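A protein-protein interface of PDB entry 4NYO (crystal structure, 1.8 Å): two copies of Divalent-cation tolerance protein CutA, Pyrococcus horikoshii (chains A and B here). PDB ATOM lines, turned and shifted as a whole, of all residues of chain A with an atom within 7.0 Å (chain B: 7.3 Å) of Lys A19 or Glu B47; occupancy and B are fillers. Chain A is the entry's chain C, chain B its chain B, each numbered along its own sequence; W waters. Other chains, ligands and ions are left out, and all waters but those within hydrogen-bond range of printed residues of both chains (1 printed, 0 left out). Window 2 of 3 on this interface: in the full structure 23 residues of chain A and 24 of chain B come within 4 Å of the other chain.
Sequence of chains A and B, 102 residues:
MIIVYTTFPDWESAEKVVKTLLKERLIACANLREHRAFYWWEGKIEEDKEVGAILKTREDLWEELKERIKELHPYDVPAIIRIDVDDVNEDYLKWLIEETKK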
ATOM      1  N   SER A  13       6.236  24.761 -13.245  1.00  0.00           N
ATOM      2  CA  SER A  13       5.169  24.918 -14.230  1.00  0.00           C
ATOM      3  C   SER A  13       3.790  24.570 -13.662  1.00  0.00           C
ATOM      4  O   SER A  13       2.806  25.260 -13.935  1.00  0.00           O
ATOM      5  CB  SER A  13       5.456  24.064 -15.471  1.00  0.00           C
ATOM      6  OG  SER A  13       5.516  22.683 -15.160  1.00  0.00           O
ATOM      7  N   ALA A  14       3.714  23.507 -12.870  1.00  0.00           N
ATOM      8  CA  ALA A  14       2.444  23.093 -12.285  1.00  0.00           C
ATOM      9  C   ALA A  14       1.814  24.220 -11.465  1.00  0.00           C
ATOM     10  O   ALA A  14       0.645  24.566 -11.660  1.00  0.00           O
ATOM     11  CB  ALA A  14       2.648  21.857 -11.410  1.00  0.00           C
ATOM     12  N   GLU A  15       2.593  24.811 -10.564  1.00  0.00           N
ATOM     13  CA  GLU A  15       2.072  25.877  -9.721  1.00  0.00           C
ATOM     14  C   GLU A  15       1.785  27.171 -10.482  1.00  0.00           C
ATOM     15  O   GLU A  15       0.798  27.851 -10.192  1.00  0.00           O
ATOM     16  CB  GLU A  15       3.017  26.140  -8.542  1.00  0.00           C
ATOM     17  CG  GLU A  15       3.208  24.928  -7.635  1.00  0.00           C
ATOM     18  CD  GLU A  15       3.731  25.290  -6.257  1.00  0.00           C
ATOM     19  OE1 GLU A  15       4.078  26.472  -6.042  1.00  0.00           O
ATOM     20  OE2 GLU A  15       3.797  24.391  -5.387  1.00  0.00           O
ATOM     21  N   LYS A  16       2.626  27.511 -11.457  1.00  0.00           N
ATOM     22  CA  LYS A  16       2.389  28.726 -12.232  1.00  0.00           C
ATOM     23  C   LYS A  16       1.081  28.603 -13.005  1.00  0.00           C
ATOM     24  O   LYS A  16       0.256  29.513 -12.993  1.00  0.00           O
ATOM     25  CB  LYS A  16       3.536  28.998 -13.215  1.00  0.00           C
ATOM     26  CG  LYS A  16       4.782  29.594 -12.570  1.00  0.00           C
ATOM     27  CD  LYS A  16       5.797  30.056 -13.613  1.00  0.00           C
ATOM     28  CE  LYS A  16       7.028  30.672 -12.955  1.00  0.00           C
ATOM     29  NZ  LYS A  16       8.068  31.053 -13.955  1.00  0.00           N
ATOM     30  N   VAL A  17       0.892  27.470 -13.673  1.00  0.00           N
ATOM     31  CA  VAL A  17      -0.322  27.256 -14.443  1.00  0.00           C
ATOM     32  C   VAL A  17      -1.552  27.248 -13.546  1.00  0.00           C
ATOM     33  O   VAL A  17      -2.510  27.973 -13.801  1.00  0.00           O
ATOM     34  CB  VAL A  17      -0.252  25.935 -15.238  1.00  0.00           C
ATOM     35  CG1 VAL A  17      -1.608  25.631 -15.871  1.00  0.00           C
ATOM     36  CG2 VAL A  17       0.811  26.047 -16.323  1.00  0.00           C
ATOM     37  N   VAL A  18      -1.519  26.439 -12.492  1.00  0.00           N
ATOM     38  CA  VAL A  18      -2.647  26.341 -11.576  1.00  0.00           C
ATOM     39  C   VAL A  18      -3.001  27.679 -10.933  1.00  0.00           C
ATOM     40  O   VAL A  18      -4.179  28.028 -10.838  1.00  0.00           O
ATOM     41  CB  VAL A  18      -2.377  25.280 -10.477  1.00  0.00           C
ATOM     42  CG1 VAL A  18      -3.421  25.371  -9.385  1.00  0.00           C
ATOM     43  CG2 VAL A  18      -2.402  23.891 -11.098  1.00  0.00           C
ATOM     44  N   LYS A  19      -1.994  28.434 -10.502  1.00  0.00           N
ATOM     45  CA  LYS A  19      -2.257  29.730  -9.890  1.00  0.00           C
ATOM     46  C   LYS A  19      -2.881  30.706 -10.885  1.00  0.00           C
ATOM     47  O   LYS A  19      -3.673  31.574 -10.497  1.00  0.00           O
ATOM     48  CB  LYS A  19      -0.971  30.314  -9.302  1.00  0.00           C
ATOM     49  CG  LYS A  19      -0.516  29.582  -8.052  1.00  0.00           C
ATOM     50  CD  LYS A  19       0.791  30.132  -7.505  1.00  0.00           C
ATOM     51  CE  LYS A  19       1.282  29.270  -6.353  1.00  0.00           C
ATOM     52  NZ  LYS A  19       2.607  29.697  -5.838  1.00  0.00           N
ATOM     53  N   THR A  20      -2.532  30.567 -12.161  1.00  0.00           N
ATOM     54  CA  THR A  20      -3.094  31.437 -13.195  1.00  0.00           C
ATOM     55  C   THR A  20      -4.569  31.083 -13.394  1.00  0.00           C
ATOM     56  O   THR A  20      -5.425  31.968 -13.518  1.00  0.00           O
ATOM     57  CB  THR A  20      -2.345  31.280 -14.540  1.00  0.00           C
ATOM     58  OG1 THR A  20      -0.987  31.708 -14.385  1.00  0.00           O
ATOM     59  CG2 THR A  20      -3.009  32.118 -15.631  1.00  0.00           C
ATOM     60  N   LEU A  21      -4.860  29.784 -13.416  1.00  0.00           N
ATOM     61  CA  LEU A  21      -6.228  29.307 -13.582  1.00  0.00           C
ATOM     62  C   LEU A  21      -7.103  29.782 -12.421  1.00  0.00           C
ATOM     63  O   LEU A  21      -8.273  30.116 -12.608  1.00  0.00           O
ATOM     64  CB  LEU A  21      -6.246  27.775 -13.656  1.00  0.00           C
ATOM     65  CG  LEU A  21      -5.495  27.179 -14.850  1.00  0.00           C
ATOM     66  CD1 LEU A  21      -5.503  25.656 -14.783  1.00  0.00           C
ATOM     67  CD2 LEU A  21      -6.143  27.662 -16.138  1.00  0.00           C
ATOM     68  N   LEU A  22      -6.533  29.801 -11.223  1.00  0.00           N
ATOM     69  CA  LEU A  22      -7.262  30.249 -10.041  1.00  0.00           C
ATOM     70  C   LEU A  22      -7.504  31.753 -10.121  1.00  0.00           C
ATOM     71  O   LEU A  22      -8.625  32.221  -9.921  1.00  0.00           O
ATOM     72  CB  LEU A  22      -6.476  29.902  -8.770  1.00  0.00           C
ATOM     73  CG  LEU A  22      -6.552  28.437  -8.316  1.00  0.00           C
ATOM     74  CD1 LEU A  22      -5.428  28.133  -7.335  1.00  0.00           C
ATOM     75  CD2 LEU A  22      -7.914  28.166  -7.678  1.00  0.00           C
ATOM     76  N   LYS A  23      -6.454  32.508 -10.437  1.00  0.00           N
ATOM     77  CA  LYS A  23      -6.566  33.960 -10.540  1.00  0.00           C
ATOM     78  C   LYS A  23      -7.655  34.370 -11.530  1.00  0.00           C
ATOM     79  O   LYS A  23      -8.367  35.354 -11.317  1.00  0.00           O
ATOM     80  CB  LYS A  23      -5.230  34.566 -10.982  1.00  0.00           C
ATOM     81  CG  LYS A  23      -5.246  36.084 -11.092  1.00  0.00           C
ATOM     82  CD  LYS A  23      -3.934  36.606 -11.676  1.00  0.00           C
ATOM     83  CE  LYS A  23      -3.899  38.130 -11.730  1.00  0.00           C
ATOM     84  NZ  LYS A  23      -3.883  38.756 -10.376  1.00  0.00           N
ATOM     85  N   GLU A  24      -7.784  33.612 -12.612  1.00  0.00           N
ATOM     86  CA  GLU A  24      -8.788  33.908 -13.623  1.00  0.00           C
ATOM     87  C   GLU A  24     -10.124  33.258 -13.272  1.00  0.00           C
ATOM     88  O   GLU A  24     -11.102  33.386 -14.010  1.00  0.00           O
ATOM     89  CB  GLU A  24      -8.293  33.438 -14.993  1.00  0.00           C
ATOM     90  CG  GLU A  24      -7.009  34.146 -15.426  1.00  0.00           C
ATOM     91  CD  GLU A  24      -6.429  33.614 -16.725  1.00  0.00           C
ATOM     92  OE1 GLU A  24      -5.378  34.136 -17.158  1.00  0.00           O
ATOM     93  OE2 GLU A  24      -7.015  32.676 -17.312  1.00  0.00           O
ATOM     94  N   ARG A  25     -10.145  32.581 -12.127  1.00  0.00           N
ATOM     95  CA  ARG A  25     -11.323  31.890 -11.610  1.00  0.00           C
ATOM     96  C   ARG A  25     -11.932  30.849 -12.546  1.00  0.00           C
ATOM     97  O   ARG A  25     -13.154  30.702 -12.625  1.00  0.00           O
ATOM     98  CB  ARG A  25     -12.384  32.905 -11.165  1.00  0.00           C
ATOM     99  CG  ARG A  25     -11.997  33.606  -9.864  1.00  0.00           C
ATOM    100  CD  ARG A  25     -13.038  34.604  -9.401  1.00  0.00           C
ATOM    101  NE  ARG A  25     -12.613  35.304  -8.191  1.00  0.00           N
ATOM    102  CZ  ARG A  25     -12.658  34.792  -6.963  1.00  0.00           C
ATOM    103  NH1 ARG A  25     -13.117  33.564  -6.764  1.00  0.00           N
ATOM    104  NH2 ARG A  25     -12.242  35.512  -5.926  1.00  0.00           N
ATOM    105  N   ILE A  27     -11.114  27.742 -12.152  1.00  0.00           N
ATOM    106  CA  ILE A  27     -11.223  26.593 -11.251  1.00  0.00           C
ATOM    107  C   ILE A  27     -11.344  27.132  -9.825  1.00  0.00           C
ATOM    108  O   ILE A  27     -10.940  28.263  -9.560  1.00  0.00           O
ATOM    109  CB  ILE A  27      -9.983  25.647 -11.352  1.00  0.00           C
ATOM    110  CG1 ILE A  27      -8.702  26.393 -10.955  1.00  0.00           C
ATOM    111  CG2 ILE A  27      -9.863  25.094 -12.775  1.00  0.00           C
ATOM    112  CD1 ILE A  27      -7.451  25.492 -10.858  1.00  0.00           C
ATOM    113  N   ARG B  36      -0.541  19.008  -2.374  1.00  0.00           N
ATOM    114  CA  ARG B  36      -0.554  20.428  -2.061  1.00  0.00           C
ATOM    115  C   ARG B  36      -1.787  21.021  -2.704  1.00  0.00           C
ATOM    116  O   ARG B  36      -1.993  20.878  -3.909  1.00  0.00           O
ATOM    117  CB  ARG B  36       0.694  21.118  -2.606  1.00  0.00           C
ATOM    118  CG  ARG B  36       1.937  20.779  -1.837  1.00  0.00           C
ATOM    119  CD  ARG B  36       3.127  21.610  -2.272  1.00  0.00           C
ATOM    120  NE  ARG B  36       4.284  21.285  -1.452  1.00  0.00           N
ATOM    121  CZ  ARG B  36       4.544  21.825  -0.267  1.00  0.00           C
ATOM    122  NH1 ARG B  36       3.737  22.741   0.247  1.00  0.00           N
ATOM    123  NH2 ARG B  36       5.599  21.421   0.418  1.00  0.00           N
ATOM    124  N   ALA B  37      -2.616  21.677  -1.902  1.00  0.00           N
ATOM    125  CA  ALA B  37      -3.827  22.269  -2.431  1.00  0.00           C
ATOM    126  C   ALA B  37      -3.724  23.776  -2.567  1.00  0.00           C
ATOM    127  O   ALA B  37      -3.107  24.453  -1.742  1.00  0.00           O
ATOM    128  CB  ALA B  37      -5.022  21.905  -1.544  1.00  0.00           C
ATOM    129  N   PHE B  38      -4.324  24.288  -3.636  1.00  0.00           N
ATOM    130  CA  PHE B  38      -4.373  25.718  -3.898  1.00  0.00           C
ATOM    131  C   PHE B  38      -5.860  25.946  -4.130  1.00  0.00           C
ATOM    132  O   PHE B  38      -6.455  25.323  -5.004  1.00  0.00           O
ATOM    133  CB  PHE B  38      -3.565  26.072  -5.153  1.00  0.00           C
ATOM    134  CG  PHE B  38      -2.114  25.693  -5.062  1.00  0.00           C
ATOM    135  CD1 PHE B  38      -1.709  24.375  -5.274  1.00  0.00           C
ATOM    136  CD2 PHE B  38      -1.151  26.646  -4.736  1.00  0.00           C
ATOM    137  CE1 PHE B  38      -0.373  24.011  -5.158  1.00  0.00           C
ATOM    138  CE2 PHE B  38       0.194  26.290  -4.616  1.00  0.00           C
ATOM    139  CZ  PHE B  38       0.584  24.971  -4.827  1.00  0.00           C
ATOM    140  N   TYR B  39      -6.463  26.823  -3.335  1.00  0.00           N
ATOM    141  CA  TYR B  39      -7.892  27.068  -3.456  1.00  0.00           C
ATOM    142  C   TYR B  39      -8.310  28.470  -3.048  1.00  0.00           C
ATOM    143  O   TYR B  39      -7.601  29.166  -2.319  1.00  0.00           O
ATOM    144  CB  TYR B  39      -8.663  26.066  -2.593  1.00  0.00           C
ATOM    145  CG  TYR B  39      -8.279  26.099  -1.135  1.00  0.00           C
ATOM    146  CD1 TYR B  39      -7.092  25.523  -0.695  1.00  0.00           C
ATOM    147  CD2 TYR B  39      -9.090  26.739  -0.197  1.00  0.00           C
ATOM    148  CE1 TYR B  39      -6.716  25.580   0.646  1.00  0.00           C
ATOM    149  CE2 TYR B  39      -8.725  26.804   1.147  1.00  0.00           C
ATOM    150  CZ  TYR B  39      -7.535  26.222   1.560  1.00  0.00           C
ATOM    151  OH  TYR B  39      -7.164  26.281   2.884  1.00  0.00           O
ATOM    152  N   TRP B  40      -9.481  28.869  -3.526  1.00  0.00           N
ATOM    153  CA  TRP B  40     -10.031  30.168  -3.200  1.00  0.00           C
ATOM    154  C   TRP B  40     -10.698  30.120  -1.833  1.00  0.00           C
ATOM    155  O   TRP B  40     -11.415  29.172  -1.518  1.00  0.00           O
ATOM    156  CB  TRP B  40     -11.071  30.580  -4.243  1.00  0.00           C
ATOM    157  CG  TRP B  40     -10.490  31.276  -5.421  1.00  0.00           C
ATOM    158  CD1 TRP B  40     -10.409  30.809  -6.696  1.00  0.00           C
ATOM    159  CD2 TRP B  40      -9.928  32.590  -5.433  1.00  0.00           C
ATOM    160  NE1 TRP B  40      -9.830  31.757  -7.512  1.00  0.00           N
ATOM    161  CE2 TRP B  40      -9.527  32.861  -6.759  1.00  0.00           C
ATOM    162  CE3 TRP B  40      -9.725  33.569  -4.450  1.00  0.00           C
ATOM    163  CZ2 TRP B  40      -8.934  34.075  -7.129  1.00  0.00           C
ATOM    164  CZ3 TRP B  40      -9.136  34.775  -4.818  1.00  0.00           C
ATOM    165  CH2 TRP B  40      -8.748  35.015  -6.148  1.00  0.00           C
ATOM    166  N   LYS B  44      -9.043  35.280  -1.216  1.00  0.00           N
ATOM    167  CA  LYS B  44      -7.608  35.009  -1.254  1.00  0.00           C
ATOM    168  C   LYS B  44      -7.331  33.574  -1.683  1.00  0.00           C
ATOM    169  O   LYS B  44      -8.074  32.663  -1.335  1.00  0.00           O
ATOM    170  CB  LYS B  44      -7.009  35.239   0.134  1.00  0.00           C
ATOM    171  CG  LYS B  44      -7.703  34.415   1.207  1.00  0.00           C
ATOM    172  CD  LYS B  44      -7.327  34.840   2.609  1.00  0.00           C
ATOM    173  CE  LYS B  44      -8.300  34.261   3.634  1.00  0.00           C
ATOM    174  NZ  LYS B  44      -8.378  32.773   3.573  1.00  0.00           N
ATOM    175  N   ILE B  45      -6.258  33.374  -2.442  1.00  0.00           N
ATOM    176  CA  ILE B  45      -5.887  32.031  -2.875  1.00  0.00           C
ATOM    177  C   ILE B  45      -5.022  31.417  -1.779  1.00  0.00           C
ATOM    178  O   ILE B  45      -3.899  31.865  -1.542  1.00  0.00           O
ATOM    179  CB  ILE B  45      -5.093  32.060  -4.201  1.00  0.00           C
ATOM    180  CG1 ILE B  45      -6.006  32.513  -5.343  1.00  0.00           C
ATOM    181  CG2 ILE B  45      -4.520  30.677  -4.500  1.00  0.00           C
ATOM    182  CD1 ILE B  45      -5.294  32.674  -6.672  1.00  0.00           C
ATOM    183  N   GLU B  46      -5.561  30.407  -1.102  1.00  0.00           N
ATOM    184  CA  GLU B  46      -4.853  29.720  -0.024  1.00  0.00           C
ATOM    185  C   GLU B  46      -3.986  28.578  -0.542  1.00  0.00           C
ATOM    186  O   GLU B  46      -4.260  27.994  -1.589  1.00  0.00           O
ATOM    187  CB  GLU B  46      -5.844  29.152   0.995  1.00  0.00           C
ATOM    188  CG  GLU B  46      -6.605  30.189   1.800  1.00  0.00           C
ATOM    189  CD  GLU B  46      -5.689  31.070   2.626  1.00  0.00           C
ATOM    190  OE1 GLU B  46      -4.784  30.529   3.294  1.00  0.00           O
ATOM    191  OE2 GLU B  46      -5.878  32.304   2.614  1.00  0.00           O
ATOM    192  N   GLU B  47      -2.943  28.264   0.218  1.00  0.00           N
ATOM    193  CA  GLU B  47      -2.021  27.191  -0.119  1.00  0.00           C
ATOM    194  C   GLU B  47      -1.880  26.332   1.141  1.00  0.00           C
ATOM    195  O   GLU B  47      -1.495  26.833   2.192  1.00  0.00           O
ATOM    196  CB  GLU B  47      -0.673  27.796  -0.518  1.00  0.00           C
ATOM    197  CG  GLU B  47       0.317  26.827  -1.119  1.00  0.00           C
ATOM    198  CD  GLU B  47       1.595  27.520  -1.562  1.00  0.00           C
ATOM    199  OE1 GLU B  47       1.515  28.437  -2.409  1.00  0.00           O
ATOM    200  OE2 GLU B  47       2.676  27.149  -1.058  1.00  0.00           O
ATOM    201  N   ASP B  48      -2.200  25.046   1.042  1.00  0.00           N
ATOM    202  CA  ASP B  48      -2.109  24.157   2.199  1.00  0.00           C
ATOM    203  C   ASP B  48      -1.755  22.726   1.846  1.00  0.00           C
ATOM    204  O   ASP B  48      -2.188  22.206   0.820  1.00  0.00           O
ATOM    205  CB  ASP B  48      -3.439  24.124   2.963  1.00  0.00           C
ATOM    206  CG  ASP B  48      -3.629  25.320   3.863  1.00  0.00           C
ATOM    207  OD1 ASP B  48      -2.788  25.522   4.764  1.00  0.00           O
ATOM    208  OD2 ASP B  48      -4.621  26.054   3.674  1.00  0.00           O
ATOM    209  N   LYS B  49      -0.959  22.092   2.702  1.00  0.00           N
ATOM    210  CA  LYS B  49      -0.616  20.695   2.501  1.00  0.00           C
ATOM    211  C   LYS B  49      -1.824  19.940   3.030  1.00  0.00           C
ATOM    212  O   LYS B  49      -2.416  20.346   4.031  1.00  0.00           O
ATOM    213  CB  LYS B  49       0.611  20.295   3.325  1.00  0.00           C
ATOM    214  CG  LYS B  49       1.912  20.920   2.880  1.00  0.00           C
ATOM    215  CD  LYS B  49       3.106  20.172   3.472  1.00  0.00           C
ATOM    216  CE  LYS B  49       3.042  20.109   4.992  1.00  0.00           C
ATOM    217  NZ  LYS B  49       3.088  21.464   5.619  1.00  0.00           N
HETATM  218  O   HOH W   1       4.222  27.181  -3.624  1.00  0.00           O
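The side-chain carboxylate of Glu B47 lies within salt-bridge range of the side-chain amino group of Lys A19, at 3.8 Å.
The indole nitrogen (NE1) of Trp B40 is in hydrogen-bond range of the backbone carbonyl oxygen (O) of Leu A22 (2.7 Å).
The side-chain amino group (NZ) of Lys A19 is in salt-bridge range of the side-chain carboxylate (OE1) of Glu A15 (3.6 Å).
Of the 14 printed residues of chain A, 6 touch a printed residue of chain B.
Of the 11 printed residues of chain B, 4 touch a printed residue of chain A.
Along chain B the printed residues that touch a printed residue of chain A span positions 38 to 47.
Among the printed residues, 9 pairs touch across the chains.
Among the printed residues, Asp or Glu carboxylates within 4 Å of a Lys or Arg side-chain nitrogen of the other chain: Lys A19 with Glu B47 (3.8 Å).
No position is printed for both chains.
Water W1 bridges the side-chain carboxylate of Glu A15 and the side-chain carboxylate of Glu B47.
Lys A19 touches two residues of chain B.
Printed residues of chain A within 4 Å of Phe B38: Glu A15 (3.3 Å), Lys A19 (3.6 Å) and Leu A22 (3.5 Å).
Of the printed residues of chain A, Trp B40 touches Leu A22, Arg A25 and Ile A27.
The nearest residue of chain B that does not touch Lys A19 is Ile B45 (4.3 Å).
The nearest residue of chain A that does not touch Glu B47 is Glu A15 (4.9 Å).
The nearest printed residue of chain A that does not touch Ile B45 is Lys A19 (4.3 Å).
OE2 of Glu A15 touches CZ of Phe B38, 3.3 Å away.
Lys A19 touches Phe B38 (CE to CE2, 3.6 Å).
Phe B38 touches Leu A22.
Leu A22 touches Ile B45.
Lys A23 touches Ile B45.
Arg A25 touches Trp B40 (NH2 to CZ3, 3.4 Å).
O of Ile A27 touches CD1 of Trp B40 (3.9 Å).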
